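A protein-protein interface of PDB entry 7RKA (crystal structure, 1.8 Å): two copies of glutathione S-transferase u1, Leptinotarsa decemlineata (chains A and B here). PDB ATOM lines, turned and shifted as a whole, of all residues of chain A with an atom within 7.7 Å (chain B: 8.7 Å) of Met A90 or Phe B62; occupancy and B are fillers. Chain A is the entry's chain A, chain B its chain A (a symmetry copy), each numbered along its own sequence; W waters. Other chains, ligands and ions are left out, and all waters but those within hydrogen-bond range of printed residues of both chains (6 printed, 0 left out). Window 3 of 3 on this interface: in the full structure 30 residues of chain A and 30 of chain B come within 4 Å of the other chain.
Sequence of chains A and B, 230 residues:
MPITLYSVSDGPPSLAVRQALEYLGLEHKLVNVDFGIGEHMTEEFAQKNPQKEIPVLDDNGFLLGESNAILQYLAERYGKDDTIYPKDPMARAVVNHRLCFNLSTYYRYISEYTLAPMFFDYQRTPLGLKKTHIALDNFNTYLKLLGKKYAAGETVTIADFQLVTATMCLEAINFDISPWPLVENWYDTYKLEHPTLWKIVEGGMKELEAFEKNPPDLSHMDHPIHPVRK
The guanidinium group (NH1) of Arg A92 is in salt-bridge range of the side-chain carboxylate (OE1) of Glu B76 (3.6 Å). The side-chain amide nitrogen (ND2) of Asn A96 sits at hydrogen-bond distance from the side-chain amide oxygen (OE1) of Gln B72 (3.4 Å).
The backbone NH (N) of Leu B64 lies within hydrogen-bond range of the backbone carbonyl oxygen (O) of Leu B57 (2.8 Å). The side-chain carboxylate of Asp A88 lies within hydrogen-bond range of the backbone NH of Met A90 (3.2 Å). The side-chain carboxylate (OD2) of Asp B59 lies within hydrogen-bond range of the side-chain hydroxyl (OH) of Tyr B73 (2.7 Å). The guanidinium group (NE) of Arg A92 sits at hydrogen-bond distance from the backbone carbonyl oxygen (O) of Pro A86 (2.8 Å).
Tyr B73 touches Pro A89. Met A90 touches Phe B62 (CE to CD1, 3.3 Å). CE1 of Tyr B73 touches CG of Met A90, 3.96 Å away. Ala A93 touches Phe B62. CB of Ala A93 touches CD2 of Leu B64, at 3.8 Å. Asn A96 touches Ala B69. Leu B64 touches His A97. His A97 touches Gly B65 (CD2 to O, 3.3 Å). His A97 touches Ala B69 (N to CB, 3.7 Å).
Met A90 touches just these residues of chain B: Phe B62 and Tyr B73. Printed residues of chain A within 4 Å of Phe B62: Met A90 (3.3 Å) and Ala A93 (3.9 Å). No residue of chain B comes within 4 Å of Ala A91. No residue of chain A comes within 4 Å of Gly B61. Printed residues of chain B within 4 Å of Arg A92: Glu B76. Printed residues of chain A within 4 Å of Glu B76: Arg A92. Of the printed residues of chain B, Asn A96 touches Ala B69 (3.9 Å) and Gln B72 (3.4 Å). Of the printed residues of chain A, Gln B72 touches Asn A96. The nearest residue of chain B that does not touch Met A90 is Arg B77 (5.4 Å). The nearest residue of chain A that does not touch Phe B62 is Val A94 (4.4 Å). The nearest printed residue of chain B that does not touch His A97 is Gln B72 (5.9 Å).
Printed residues of chain B that touch a printed residue of chain A: Phe B62, Leu B64, Gly B65, Ala B69, Gln B72, Tyr B73 and Glu B76. Hydrophobic or aromatic side chains of chain B within 4 Å of the printed part of chain A: Phe B62, Leu B64, Ala B69 and Tyr B73. Among the printed residues, Asp or Glu carboxylates within 4 Å of a Lys or Arg side-chain nitrogen of the other chain: Arg A92 with Glu B76 (3.6 Å).
No position is printed for both chains.
Water W3 bridges the side-chain carboxylate of Glu B76 and the side-chain amide nitrogen of Asn A96. Water W1 bridges O of Pro A89 and OE2 of Glu B76. Water W2 bridges the side-chain amide oxygen of Gln B72 (2.9 Å) and the backbone carbonyl oxygen of Asn A96 (3.4 Å). Water W6 lies within hydrogen-bond range of the backbone carbonyl oxygen (O) of Ala B69 (2.9 Å), the side-chain amide nitrogen (ND2) of Asn A96 (2.9 Å) and the backbone NH (N) of Tyr B73 (3.4 Å). Water W4 lies within hydrogen-bond range of the backbone NH of Gly B65 and a ring nitrogen (NE2) of His A97.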
ATOM      1  N   PRO A  86       3.195 -14.617  -2.454  1.00  0.00           N
ATOM      2  CA  PRO A  86       2.650 -13.398  -3.062  1.00  0.00           C
ATOM      3  C   PRO A  86       2.080 -13.630  -4.453  1.00  0.00           C
ATOM      4  O   PRO A  86       2.573 -14.451  -5.227  1.00  0.00           O
ATOM      5  CB  PRO A  86       3.851 -12.447  -3.128  1.00  0.00           C
ATOM      6  CG  PRO A  86       4.914 -13.044  -2.376  1.00  0.00           C
ATOM      7  CD  PRO A  86       4.618 -14.478  -2.083  1.00  0.00           C
ATOM      8  N   LYS A  87       1.030 -12.864  -4.768  1.00  0.00           N
ATOM      9  CA  LYS A  87       0.365 -12.992  -6.062  1.00  0.00           C
ATOM     10  C   LYS A  87       1.107 -12.264  -7.174  1.00  0.00           C
ATOM     11  O   LYS A  87       1.026 -12.672  -8.345  1.00  0.00           O
ATOM     12  CB  LYS A  87      -1.073 -12.477  -5.950  1.00  0.00           C
ATOM     13  CG  LYS A  87      -1.891 -13.236  -4.920  1.00  0.00           C
ATOM     14  CD  LYS A  87      -3.296 -13.530  -5.381  1.00  0.00           C
ATOM     15  CE  LYS A  87      -4.071 -14.240  -4.280  1.00  0.00           C
ATOM     16  NZ  LYS A  87      -3.700 -15.699  -4.139  1.00  0.00           N
ATOM     17  N   ASP A  88       1.825 -11.204  -6.848  1.00  0.00           N
ATOM     18  CA  ASP A  88       2.567 -10.481  -7.863  1.00  0.00           C
ATOM     19  C   ASP A  88       3.473 -11.451  -8.614  1.00  0.00           C
ATOM     20  O   ASP A  88       4.261 -12.160  -7.975  1.00  0.00           O
ATOM     21  CB  ASP A  88       3.420  -9.380  -7.236  1.00  0.00           C
ATOM     22  CG  ASP A  88       4.356  -8.731  -8.247  1.00  0.00           C
ATOM     23  OD1 ASP A  88       3.856  -7.923  -9.060  1.00  0.00           O
ATOM     24  OD2 ASP A  88       5.575  -9.026  -8.239  1.00  0.00           O
ATOM     25  N   PRO A  89       3.442 -11.471  -9.958  1.00  0.00           N
ATOM     26  CA  PRO A  89       4.212 -12.506 -10.679  1.00  0.00           C
ATOM     27  C   PRO A  89       5.699 -12.484 -10.376  1.00  0.00           C
ATOM     28  O   PRO A  89       6.292 -13.554 -10.236  1.00  0.00           O
ATOM     29  CB  PRO A  89       3.925 -12.209 -12.162  1.00  0.00           C
ATOM     30  CG  PRO A  89       2.611 -11.472 -12.156  1.00  0.00           C
ATOM     31  CD  PRO A  89       2.566 -10.692 -10.857  1.00  0.00           C
ATOM     32  N   MET A  90       6.332 -11.317 -10.275  1.00  0.00           N
ATOM     33  CA  MET A  90       7.768 -11.279 -10.006  1.00  0.00           C
ATOM     34  C   MET A  90       8.089 -11.716  -8.576  1.00  0.00           C
ATOM     35  O   MET A  90       9.020 -12.505  -8.345  1.00  0.00           O
ATOM     36  CB  MET A  90       8.308  -9.869 -10.263  1.00  0.00           C
ATOM     37  CG  MET A  90       8.418  -9.498 -11.729  1.00  0.00           C
ATOM     38  SD  MET A  90       9.335  -7.952 -12.030  1.00  0.00           S
ATOM     39  CE  MET A  90      10.772  -8.156 -11.002  1.00  0.00           C
ATOM     40  N   ALA A  91       7.333 -11.222  -7.598  1.00  0.00           N
ATOM     41  CA  ALA A  91       7.541 -11.686  -6.228  1.00  0.00           C
ATOM     42  C   ALA A  91       7.272 -13.177  -6.115  1.00  0.00           C
ATOM     43  O   ALA A  91       8.007 -13.904  -5.428  1.00  0.00           O
ATOM     44  CB  ALA A  91       6.634 -10.939  -5.252  1.00  0.00           C
ATOM     45  N   ARG A  92       6.214 -13.650  -6.770  1.00  0.00           N
ATOM     46  CA  ARG A  92       5.924 -15.077  -6.734  1.00  0.00           C
ATOM     47  C   ARG A  92       7.042 -15.894  -7.381  1.00  0.00           C
ATOM     48  O   ARG A  92       7.347 -17.005  -6.928  1.00  0.00           O
ATOM     49  CB  ARG A  92       4.598 -15.373  -7.419  1.00  0.00           C
ATOM     50  CG  ARG A  92       4.358 -16.913  -7.436  1.00  0.00           C
ATOM     51  CD  ARG A  92       2.975 -17.267  -7.652  1.00  0.00           C
ATOM     52  NE  ARG A  92       2.135 -16.864  -6.541  1.00  0.00           N
ATOM     53  CZ  ARG A  92       0.870 -17.210  -6.463  1.00  0.00           C
ATOM     54  NH1 ARG A  92       0.360 -17.978  -7.419  1.00  0.00           N
ATOM     55  NH2 ARG A  92       0.132 -16.795  -5.453  1.00  0.00           N
ATOM     56  N   ALA A  93       7.646 -15.373  -8.456  1.00  0.00           N
ATOM     57  CA  ALA A  93       8.681 -16.117  -9.156  1.00  0.00           C
ATOM     58  C   ALA A  93       9.888 -16.373  -8.258  1.00  0.00           C
ATOM     59  O   ALA A  93      10.503 -17.441  -8.345  1.00  0.00           O
ATOM     60  CB  ALA A  93       9.085 -15.379 -10.430  1.00  0.00           C
ATOM     61  N   VAL A  94      10.219 -15.444  -7.367  1.00  0.00           N
ATOM     62  CA  VAL A  94      11.322 -15.699  -6.438  1.00  0.00           C
ATOM     63  C   VAL A  94      10.968 -16.846  -5.490  1.00  0.00           C
ATOM     64  O   VAL A  94      11.807 -17.709  -5.213  1.00  0.00           O
ATOM     65  CB  VAL A  94      11.691 -14.424  -5.663  1.00  0.00           C
ATOM     66  CG1 VAL A  94      12.837 -14.693  -4.706  1.00  0.00           C
ATOM     67  CG2 VAL A  94      12.089 -13.301  -6.629  1.00  0.00           C
ATOM     68  N   VAL A  95       9.724 -16.886  -4.993  1.00  0.00           N
ATOM     69  CA  VAL A  95       9.317 -18.021  -4.159  1.00  0.00           C
ATOM     70  C   VAL A  95       9.396 -19.316  -4.952  1.00  0.00           C
ATOM     71  O   VAL A  95       9.923 -20.329  -4.466  1.00  0.00           O
ATOM     72  CB  VAL A  95       7.905 -17.820  -3.577  1.00  0.00           C
ATOM     73  CG1 VAL A  95       7.533 -19.007  -2.662  1.00  0.00           C
ATOM     74  CG2 VAL A  95       7.784 -16.497  -2.782  1.00  0.00           C
ATOM     75  N   ASN A  96       8.860 -19.307  -6.180  1.00  0.00           N
ATOM     76  CA  ASN A  96       8.839 -20.522  -7.001  1.00  0.00           C
ATOM     77  C   ASN A  96      10.253 -20.977  -7.321  1.00  0.00           C
ATOM     78  O   ASN A  96      10.540 -22.189  -7.358  1.00  0.00           O
ATOM     79  CB  ASN A  96       8.049 -20.286  -8.299  1.00  0.00           C
ATOM     80  CG  ASN A  96       6.530 -20.285  -8.094  1.00  0.00           C
ATOM     81  OD1 ASN A  96       5.999 -20.769  -7.086  1.00  0.00           O
ATOM     82  ND2 ASN A  96       5.826 -19.729  -9.057  1.00  0.00           N
ATOM     83  N   HIS A  97      11.148 -20.023  -7.555  1.00  0.00           N
ATOM     84  CA  HIS A  97      12.529 -20.381  -7.838  1.00  0.00           C
ATOM     85  C   HIS A  97      13.148 -21.097  -6.652  1.00  0.00           C
ATOM     86  O   HIS A  97      13.783 -22.138  -6.815  1.00  0.00           O
ATOM     87  CB  HIS A  97      13.371 -19.172  -8.189  1.00  0.00           C
ATOM     88  CG  HIS A  97      14.826 -19.506  -8.286  1.00  0.00           C
ATOM     89  ND1 HIS A  97      15.657 -19.508  -7.186  1.00  0.00           N
ATOM     90  CD2 HIS A  97      15.565 -19.969  -9.320  1.00  0.00           C
ATOM     91  CE1 HIS A  97      16.865 -19.904  -7.552  1.00  0.00           C
ATOM     92  NE2 HIS A  97      16.837 -20.179  -8.846  1.00  0.00           N
ATOM     93  N   LEU A 146      19.651 -11.675  -3.205  1.00  0.00           N
ATOM     94  CA  LEU A 146      18.362 -11.048  -2.931  1.00  0.00           C
ATOM     95  C   LEU A 146      18.476  -9.969  -1.858  1.00  0.00           C
ATOM     96  O   LEU A 146      17.790  -8.939  -1.927  1.00  0.00           O
ATOM     97  CB  LEU A 146      17.340 -12.109  -2.508  1.00  0.00           C
ATOM     98  CG  LEU A 146      15.872 -11.673  -2.488  1.00  0.00           C
ATOM     99  CD1 LEU A 146      15.363 -11.323  -3.901  1.00  0.00           C
ATOM    100  CD2 LEU A 146      14.976 -12.771  -1.861  1.00  0.00           C
ATOM    101  N   ALA A 152      12.955 -15.753   0.271  1.00  0.00           N
ATOM    102  CA  ALA A 152      12.298 -15.217  -0.909  1.00  0.00           C
ATOM    103  C   ALA A 152      11.560 -13.934  -0.604  1.00  0.00           C
ATOM    104  O   ALA A 152      10.554 -13.640  -1.250  1.00  0.00           O
ATOM    105  CB  ALA A 152      11.317 -16.228  -1.519  1.00  0.00           C
ATOM    106  N   PRO B   2      13.538  -5.630 -23.350  1.00  0.00           N
ATOM    107  CA  PRO B   2      13.406  -6.890 -24.094  1.00  0.00           C
ATOM    108  C   PRO B   2      13.546  -8.138 -23.219  1.00  0.00           C
ATOM    109  O   PRO B   2      13.895  -8.049 -22.046  1.00  0.00           O
ATOM    110  CB  PRO B   2      14.558  -6.826 -25.111  1.00  0.00           C
ATOM    111  CG  PRO B   2      15.525  -5.745 -24.583  1.00  0.00           C
ATOM    112  CD  PRO B   2      14.924  -5.139 -23.330  1.00  0.00           C
ATOM    113  N   ILE B   3      13.258  -9.298 -23.800  1.00  0.00           N
ATOM    114  CA  ILE B   3      13.425 -10.584 -23.134  1.00  0.00           C
ATOM    115  C   ILE B   3      14.593 -11.316 -23.787  1.00  0.00           C
ATOM    116  O   ILE B   3      14.678 -11.398 -25.018  1.00  0.00           O
ATOM    117  CB  ILE B   3      12.138 -11.426 -23.214  1.00  0.00           C
ATOM    118  CG1 ILE B   3      10.994 -10.737 -22.465  1.00  0.00           C
ATOM    119  CG2 ILE B   3      12.412 -12.826 -22.652  1.00  0.00           C
ATOM    120  CD1 ILE B   3       9.649 -11.444 -22.610  1.00  0.00           C
ATOM    121  N   THR B   4      15.471 -11.873 -22.968  1.00  0.00           N
ATOM    122  CA  THR B   4      16.565 -12.706 -23.437  1.00  0.00           C
ATOM    123  C   THR B   4      16.476 -14.042 -22.717  1.00  0.00           C
ATOM    124  O   THR B   4      16.299 -14.077 -21.494  1.00  0.00           O
ATOM    125  CB  THR B   4      17.931 -12.074 -23.160  1.00  0.00           C
ATOM    126  OG1 THR B   4      18.035 -10.822 -23.845  1.00  0.00           O
ATOM    127  CG2 THR B   4      19.046 -12.976 -23.621  1.00  0.00           C
ATOM    128  N   TYR B   6      18.815 -17.290 -22.036  1.00  0.00           N
ATOM    129  CA  TYR B   6      20.079 -17.999 -22.065  1.00  0.00           C
ATOM    130  C   TYR B   6      19.777 -19.486 -21.995  1.00  0.00           C
ATOM    131  O   TYR B   6      19.131 -19.942 -21.048  1.00  0.00           O
ATOM    132  CB  TYR B   6      20.964 -17.557 -20.911  1.00  0.00           C
ATOM    133  CG  TYR B   6      21.318 -16.090 -21.038  1.00  0.00           C
ATOM    134  CD1 TYR B   6      20.496 -15.115 -20.509  1.00  0.00           C
ATOM    135  CD2 TYR B   6      22.458 -15.685 -21.732  1.00  0.00           C
ATOM    136  CE1 TYR B   6      20.804 -13.770 -20.637  1.00  0.00           C
ATOM    137  CE2 TYR B   6      22.768 -14.350 -21.865  1.00  0.00           C
ATOM    138  CZ  TYR B   6      21.935 -13.397 -21.320  1.00  0.00           C
ATOM    139  OH  TYR B   6      22.238 -12.053 -21.444  1.00  0.00           O
ATOM    140  N   PHE B  45      26.717 -11.930 -15.998  1.00  0.00           N
ATOM    141  CA  PHE B  45      25.891 -12.215 -14.829  1.00  0.00           C
ATOM    142  C   PHE B  45      26.170 -13.600 -14.250  1.00  0.00           C
ATOM    143  O   PHE B  45      25.244 -14.302 -13.833  1.00  0.00           O
ATOM    144  CB  PHE B  45      24.400 -12.043 -15.188  1.00  0.00           C
ATOM    145  CG  PHE B  45      23.856 -13.107 -16.123  1.00  0.00           C
ATOM    146  CD1 PHE B  45      22.975 -14.064 -15.670  1.00  0.00           C
ATOM    147  CD2 PHE B  45      24.210 -13.126 -17.458  1.00  0.00           C
ATOM    148  CE1 PHE B  45      22.479 -15.033 -16.525  1.00  0.00           C
ATOM    149  CE2 PHE B  45      23.714 -14.096 -18.312  1.00  0.00           C
ATOM    150  CZ  PHE B  45      22.857 -15.054 -17.842  1.00  0.00           C
ATOM    151  N   VAL B  56      18.407 -19.429 -18.066  1.00  0.00           N
ATOM    152  CA  VAL B  56      18.100 -18.238 -17.289  1.00  0.00           C
ATOM    153  C   VAL B  56      17.336 -17.290 -18.190  1.00  0.00           C
ATOM    154  O   VAL B  56      17.750 -17.046 -19.328  1.00  0.00           O
ATOM    155  CB  VAL B  56      19.365 -17.545 -16.742  1.00  0.00           C
ATOM    156  CG1 VAL B  56      18.982 -16.181 -16.167  1.00  0.00           C
ATOM    157  CG2 VAL B  56      20.014 -18.410 -15.700  1.00  0.00           C
ATOM    158  N   LEU B  57      16.220 -16.767 -17.686  1.00  0.00           N
ATOM    159  CA  LEU B  57      15.425 -15.774 -18.380  1.00  0.00           C
ATOM    160  C   LEU B  57      15.797 -14.389 -17.872  1.00  0.00           C
ATOM    161  O   LEU B  57      15.815 -14.160 -16.658  1.00  0.00           O
ATOM    162  CB  LEU B  57      13.928 -15.999 -18.152  1.00  0.00           C
ATOM    163  CG  LEU B  57      12.986 -15.077 -18.921  1.00  0.00           C
ATOM    164  CD1 LEU B  57      12.762 -15.620 -20.330  1.00  0.00           C
ATOM    165  CD2 LEU B  57      11.630 -14.891 -18.219  1.00  0.00           C
ATOM    166  N   ASP B  58      16.035 -13.460 -18.798  1.00  0.00           N
ATOM    167  CA  ASP B  58      16.238 -12.041 -18.471  1.00  0.00           C
ATOM    168  C   ASP B  58      15.044 -11.267 -19.026  1.00  0.00           C
ATOM    169  O   ASP B  58      14.986 -10.960 -20.221  1.00  0.00           O
ATOM    170  CB  ASP B  58      17.570 -11.537 -19.026  1.00  0.00           C
ATOM    171  CG  ASP B  58      17.847 -10.067 -18.672  1.00  0.00           C
ATOM    172  OD1 ASP B  58      16.938  -9.363 -18.171  1.00  0.00           O
ATOM    173  OD2 ASP B  58      18.998  -9.638 -18.874  1.00  0.00           O
ATOM    174  N   ASP B  59      14.078 -10.965 -18.158  1.00  0.00           N
ATOM    175  CA  ASP B  59      12.903 -10.188 -18.547  1.00  0.00           C
ATOM    176  C   ASP B  59      13.141  -8.736 -18.120  1.00  0.00           C
ATOM    177  O   ASP B  59      12.891  -8.354 -16.975  1.00  0.00           O
ATOM    178  CB  ASP B  59      11.622 -10.746 -17.932  1.00  0.00           C
ATOM    179  CG  ASP B  59      10.362 -10.057 -18.463  1.00  0.00           C
ATOM    180  OD1 ASP B  59      10.490  -9.011 -19.141  1.00  0.00           O
ATOM    181  OD2 ASP B  59       9.230 -10.552 -18.215  1.00  0.00           O
ATOM    182  N   ASN B  60      13.673  -7.930 -19.042  1.00  0.00           N
ATOM    183  CA  ASN B  60      13.821  -6.493 -18.809  1.00  0.00           C
ATOM    184  C   ASN B  60      14.567  -6.206 -17.513  1.00  0.00           C
ATOM    185  O   ASN B  60      14.205  -5.308 -16.750  1.00  0.00           O
ATOM    186  CB  ASN B  60      12.452  -5.830 -18.800  1.00  0.00           C
ATOM    187  CG  ASN B  60      11.828  -5.766 -20.177  1.00  0.00           C
ATOM    188  OD1 ASN B  60      12.427  -5.226 -21.113  1.00  0.00           O
ATOM    189  ND2 ASN B  60      10.634  -6.351 -20.323  1.00  0.00           N
ATOM    190  N   GLY B  61      15.617  -6.985 -17.261  1.00  0.00           N
ATOM    191  CA  GLY B  61      16.449  -6.838 -16.089  1.00  0.00           C
ATOM    192  C   GLY B  61      16.133  -7.790 -14.946  1.00  0.00           C
ATOM    193  O   GLY B  61      16.948  -7.914 -14.026  1.00  0.00           O
ATOM    194  N   PHE B  62      14.975  -8.442 -14.971  1.00  0.00           N
ATOM    195  CA  PHE B  62      14.593  -9.428 -13.957  1.00  0.00           C
ATOM    196  C   PHE B  62      15.158 -10.774 -14.403  1.00  0.00           C
ATOM    197  O   PHE B  62      14.741 -11.311 -15.436  1.00  0.00           O
ATOM    198  CB  PHE B  62      13.071  -9.475 -13.799  1.00  0.00           C
ATOM    199  CG  PHE B  62      12.585 -10.552 -12.835  1.00  0.00           C
ATOM    200  CD1 PHE B  62      13.010 -10.564 -11.505  1.00  0.00           C
ATOM    201  CD2 PHE B  62      11.723 -11.548 -13.262  1.00  0.00           C
ATOM    202  CE1 PHE B  62      12.592 -11.548 -10.627  1.00  0.00           C
ATOM    203  CE2 PHE B  62      11.276 -12.536 -12.371  1.00  0.00           C
ATOM    204  CZ  PHE B  62      11.723 -12.535 -11.063  1.00  0.00           C
ATOM    205  N   LEU B  63      16.122 -11.302 -13.652  1.00  0.00           N
ATOM    206  CA  LEU B  63      16.795 -12.555 -13.992  1.00  0.00           C
ATOM    207  C   LEU B  63      16.186 -13.718 -13.210  1.00  0.00           C
ATOM    208  O   LEU B  63      16.144 -13.688 -11.975  1.00  0.00           O
ATOM    209  CB  LEU B  63      18.293 -12.460 -13.705  1.00  0.00           C
ATOM    210  CG  LEU B  63      19.098 -11.491 -14.572  1.00  0.00           C
ATOM    211  CD1 LEU B  63      20.475 -11.255 -13.958  1.00  0.00           C
ATOM    212  CD2 LEU B  63      19.226 -12.036 -15.994  1.00  0.00           C
ATOM    213  N   LEU B  64      15.714 -14.742 -13.922  1.00  0.00           N
ATOM    214  CA  LEU B  64      15.031 -15.865 -13.282  1.00  0.00           C
ATOM    215  C   LEU B  64      15.537 -17.194 -13.829  1.00  0.00           C
ATOM    216  O   LEU B  64      15.478 -17.428 -15.042  1.00  0.00           O
ATOM    217  CB  LEU B  64      13.527 -15.744 -13.505  1.00  0.00           C
ATOM    218  CG  LEU B  64      12.660 -16.846 -12.920  1.00  0.00           C
ATOM    219  CD1 LEU B  64      12.783 -16.886 -11.401  1.00  0.00           C
ATOM    220  CD2 LEU B  64      11.222 -16.638 -13.328  1.00  0.00           C
ATOM    221  N   GLY B  65      16.051 -18.051 -12.944  1.00  0.00           N
ATOM    222  CA  GLY B  65      16.427 -19.405 -13.290  1.00  0.00           C
ATOM    223  C   GLY B  65      15.361 -20.411 -12.878  1.00  0.00           C
ATOM    224  O   GLY B  65      14.291 -20.054 -12.386  1.00  0.00           O
ATOM    225  N   ALA B  69      10.072 -22.585 -12.689  1.00  0.00           N
ATOM    226  CA  ALA B  69       9.713 -21.246 -12.225  1.00  0.00           C
ATOM    227  C   ALA B  69       9.619 -20.261 -13.391  1.00  0.00           C
ATOM    228  O   ALA B  69       8.752 -19.370 -13.394  1.00  0.00           O
ATOM    229  CB  ALA B  69      10.736 -20.736 -11.200  1.00  0.00           C
ATOM    230  N   ILE B  70      10.509 -20.398 -14.381  1.00  0.00           N
ATOM    231  CA  ILE B  70      10.399 -19.579 -15.590  1.00  0.00           C
ATOM    232  C   ILE B  70       9.048 -19.799 -16.264  1.00  0.00           C
ATOM    233  O   ILE B  70       8.372 -18.845 -16.667  1.00  0.00           O
ATOM    234  CB  ILE B  70      11.558 -19.874 -16.551  1.00  0.00           C
ATOM    235  CG1 ILE B  70      12.893 -19.486 -15.924  1.00  0.00           C
ATOM    236  CG2 ILE B  70      11.343 -19.131 -17.861  1.00  0.00           C
ATOM    237  CD1 ILE B  70      14.104 -20.140 -16.613  1.00  0.00           C
ATOM    238  N   GLN B  72       6.192 -20.987 -14.952  1.00  0.00           N
ATOM    239  CA  GLN B  72       5.135 -20.472 -14.101  1.00  0.00           C
ATOM    240  C   GLN B  72       5.039 -18.952 -14.184  1.00  0.00           C
ATOM    241  O   GLN B  72       3.936 -18.401 -14.162  1.00  0.00           O
ATOM    242  CB  GLN B  72       5.370 -20.917 -12.650  1.00  0.00           C
ATOM    243  CG  GLN B  72       5.191 -22.423 -12.452  1.00  0.00           C
ATOM    244  CD  GLN B  72       5.818 -22.962 -11.168  1.00  0.00           C
ATOM    245  OE1 GLN B  72       6.872 -22.500 -10.720  1.00  0.00           O
ATOM    246  NE2 GLN B  72       5.205 -24.017 -10.623  1.00  0.00           N
ATOM    247  N   TYR B  73       6.180 -18.276 -14.285  1.00  0.00           N
ATOM    248  CA  TYR B  73       6.221 -16.817 -14.405  1.00  0.00           C
ATOM    249  C   TYR B  73       5.703 -16.359 -15.763  1.00  0.00           C
ATOM    250  O   TYR B  73       4.837 -15.469 -15.845  1.00  0.00           O
ATOM    251  CB  TYR B  73       7.666 -16.334 -14.200  1.00  0.00           C
ATOM    252  CG  TYR B  73       7.885 -14.892 -14.615  1.00  0.00           C
ATOM    253  CD1 TYR B  73       7.492 -13.860 -13.785  1.00  0.00           C
ATOM    254  CD2 TYR B  73       8.478 -14.569 -15.836  1.00  0.00           C
ATOM    255  CE1 TYR B  73       7.659 -12.531 -14.153  1.00  0.00           C
ATOM    256  CE2 TYR B  73       8.664 -13.220 -16.214  1.00  0.00           C
ATOM    257  CZ  TYR B  73       8.243 -12.219 -15.364  1.00  0.00           C
ATOM    258  OH  TYR B  73       8.392 -10.883 -15.711  1.00  0.00           O
ATOM    259  N   LEU B  74       6.221 -16.952 -16.841  1.00  0.00           N
ATOM    260  CA  LEU B  74       5.800 -16.528 -18.176  1.00  0.00           C
ATOM    261  C   LEU B  74       4.303 -16.697 -18.356  1.00  0.00           C
ATOM    262  O   LEU B  74       3.631 -15.822 -18.920  1.00  0.00           O
ATOM    263  CB  LEU B  74       6.541 -17.321 -19.255  1.00  0.00           C
ATOM    264  CG  LEU B  74       8.030 -17.057 -19.477  1.00  0.00           C
ATOM    265  CD1 LEU B  74       8.573 -18.101 -20.468  1.00  0.00           C
ATOM    266  CD2 LEU B  74       8.260 -15.639 -19.986  1.00  0.00           C
ATOM    267  N   GLU B  76       1.897 -16.861 -16.038  1.00  0.00           N
ATOM    268  CA  GLU B  76       1.065 -15.956 -15.242  1.00  0.00           C
ATOM    269  C   GLU B  76       1.140 -14.515 -15.744  1.00  0.00           C
ATOM    270  O   GLU B  76       0.143 -13.790 -15.696  1.00  0.00           O
ATOM    271  CB  GLU B  76       1.460 -15.971 -13.762  1.00  0.00           C
ATOM    272  CG  GLU B  76       1.378 -17.330 -13.105  1.00  0.00           C
ATOM    273  CD  GLU B  76       1.770 -17.284 -11.637  1.00  0.00           C
ATOM    274  OE1 GLU B  76       0.877 -16.889 -10.837  1.00  0.00           O
ATOM    275  OE2 GLU B  76       2.952 -17.599 -11.310  1.00  0.00           O
ATOM    276  N   ARG B  77       2.324 -14.071 -16.176  1.00  0.00           N
ATOM    277  CA  ARG B  77       2.555 -12.672 -16.531  1.00  0.00           C
ATOM    278  C   ARG B  77       2.088 -12.335 -17.941  1.00  0.00           C
ATOM    279  O   ARG B  77       1.685 -11.192 -18.188  1.00  0.00           O
ATOM    280  CB  ARG B  77       4.047 -12.373 -16.384  1.00  0.00           C
ATOM    281  CG  ARG B  77       4.573 -10.983 -16.767  1.00  0.00           C
ATOM    282  CD  ARG B  77       3.827  -9.844 -16.117  1.00  0.00           C
ATOM    283  NE  ARG B  77       3.886  -8.661 -16.979  1.00  0.00           N
ATOM    284  CZ  ARG B  77       4.945  -7.866 -17.078  1.00  0.00           C
ATOM    285  NH1 ARG B  77       6.031  -8.126 -16.360  1.00  0.00           N
ATOM    286  NH2 ARG B  77       4.916  -6.815 -17.893  1.00  0.00           N
ATOM    287  N   TYR B  78       2.110 -13.299 -18.867  1.00  0.00           N
ATOM    288  CA  TYR B  78       1.798 -13.033 -20.268  1.00  0.00           C
ATOM    289  C   TYR B  78       0.681 -13.936 -20.787  1.00  0.00           C
ATOM    290  O   TYR B  78       0.328 -14.959 -20.200  1.00  0.00           O
ATOM    291  CB  TYR B  78       3.056 -13.192 -21.127  1.00  0.00           C
ATOM    292  CG  TYR B  78       4.162 -12.271 -20.738  1.00  0.00           C
ATOM    293  CD1 TYR B  78       4.033 -10.895 -20.908  1.00  0.00           C
ATOM    294  CD2 TYR B  78       5.338 -12.761 -20.180  1.00  0.00           C
ATOM    295  CE1 TYR B  78       5.047 -10.036 -20.549  1.00  0.00           C
ATOM    296  CE2 TYR B  78       6.363 -11.909 -19.824  1.00  0.00           C
ATOM    297  CZ  TYR B  78       6.203 -10.538 -20.011  1.00  0.00           C
ATOM    298  OH  TYR B  78       7.198  -9.677 -19.664  1.00  0.00           O
HETATM  299  O   HOH W   1       5.490 -16.098 -11.252  1.00  0.00           O
HETATM  300  O   HOH W   2       7.816 -23.848  -8.384  1.00  0.00           O
HETATM  301  O   HOH W   3       2.879 -19.831  -9.542  1.00  0.00           O
HETATM  302  O   HOH W   4      17.104 -17.033 -10.316  1.00  0.00           O
HETATM  303  O   HOH W   5       0.258 -14.915  -9.419  1.00  0.00           O
HETATM  304  O   HOH W   6       7.332 -18.405 -11.102  1.00  0.00           O
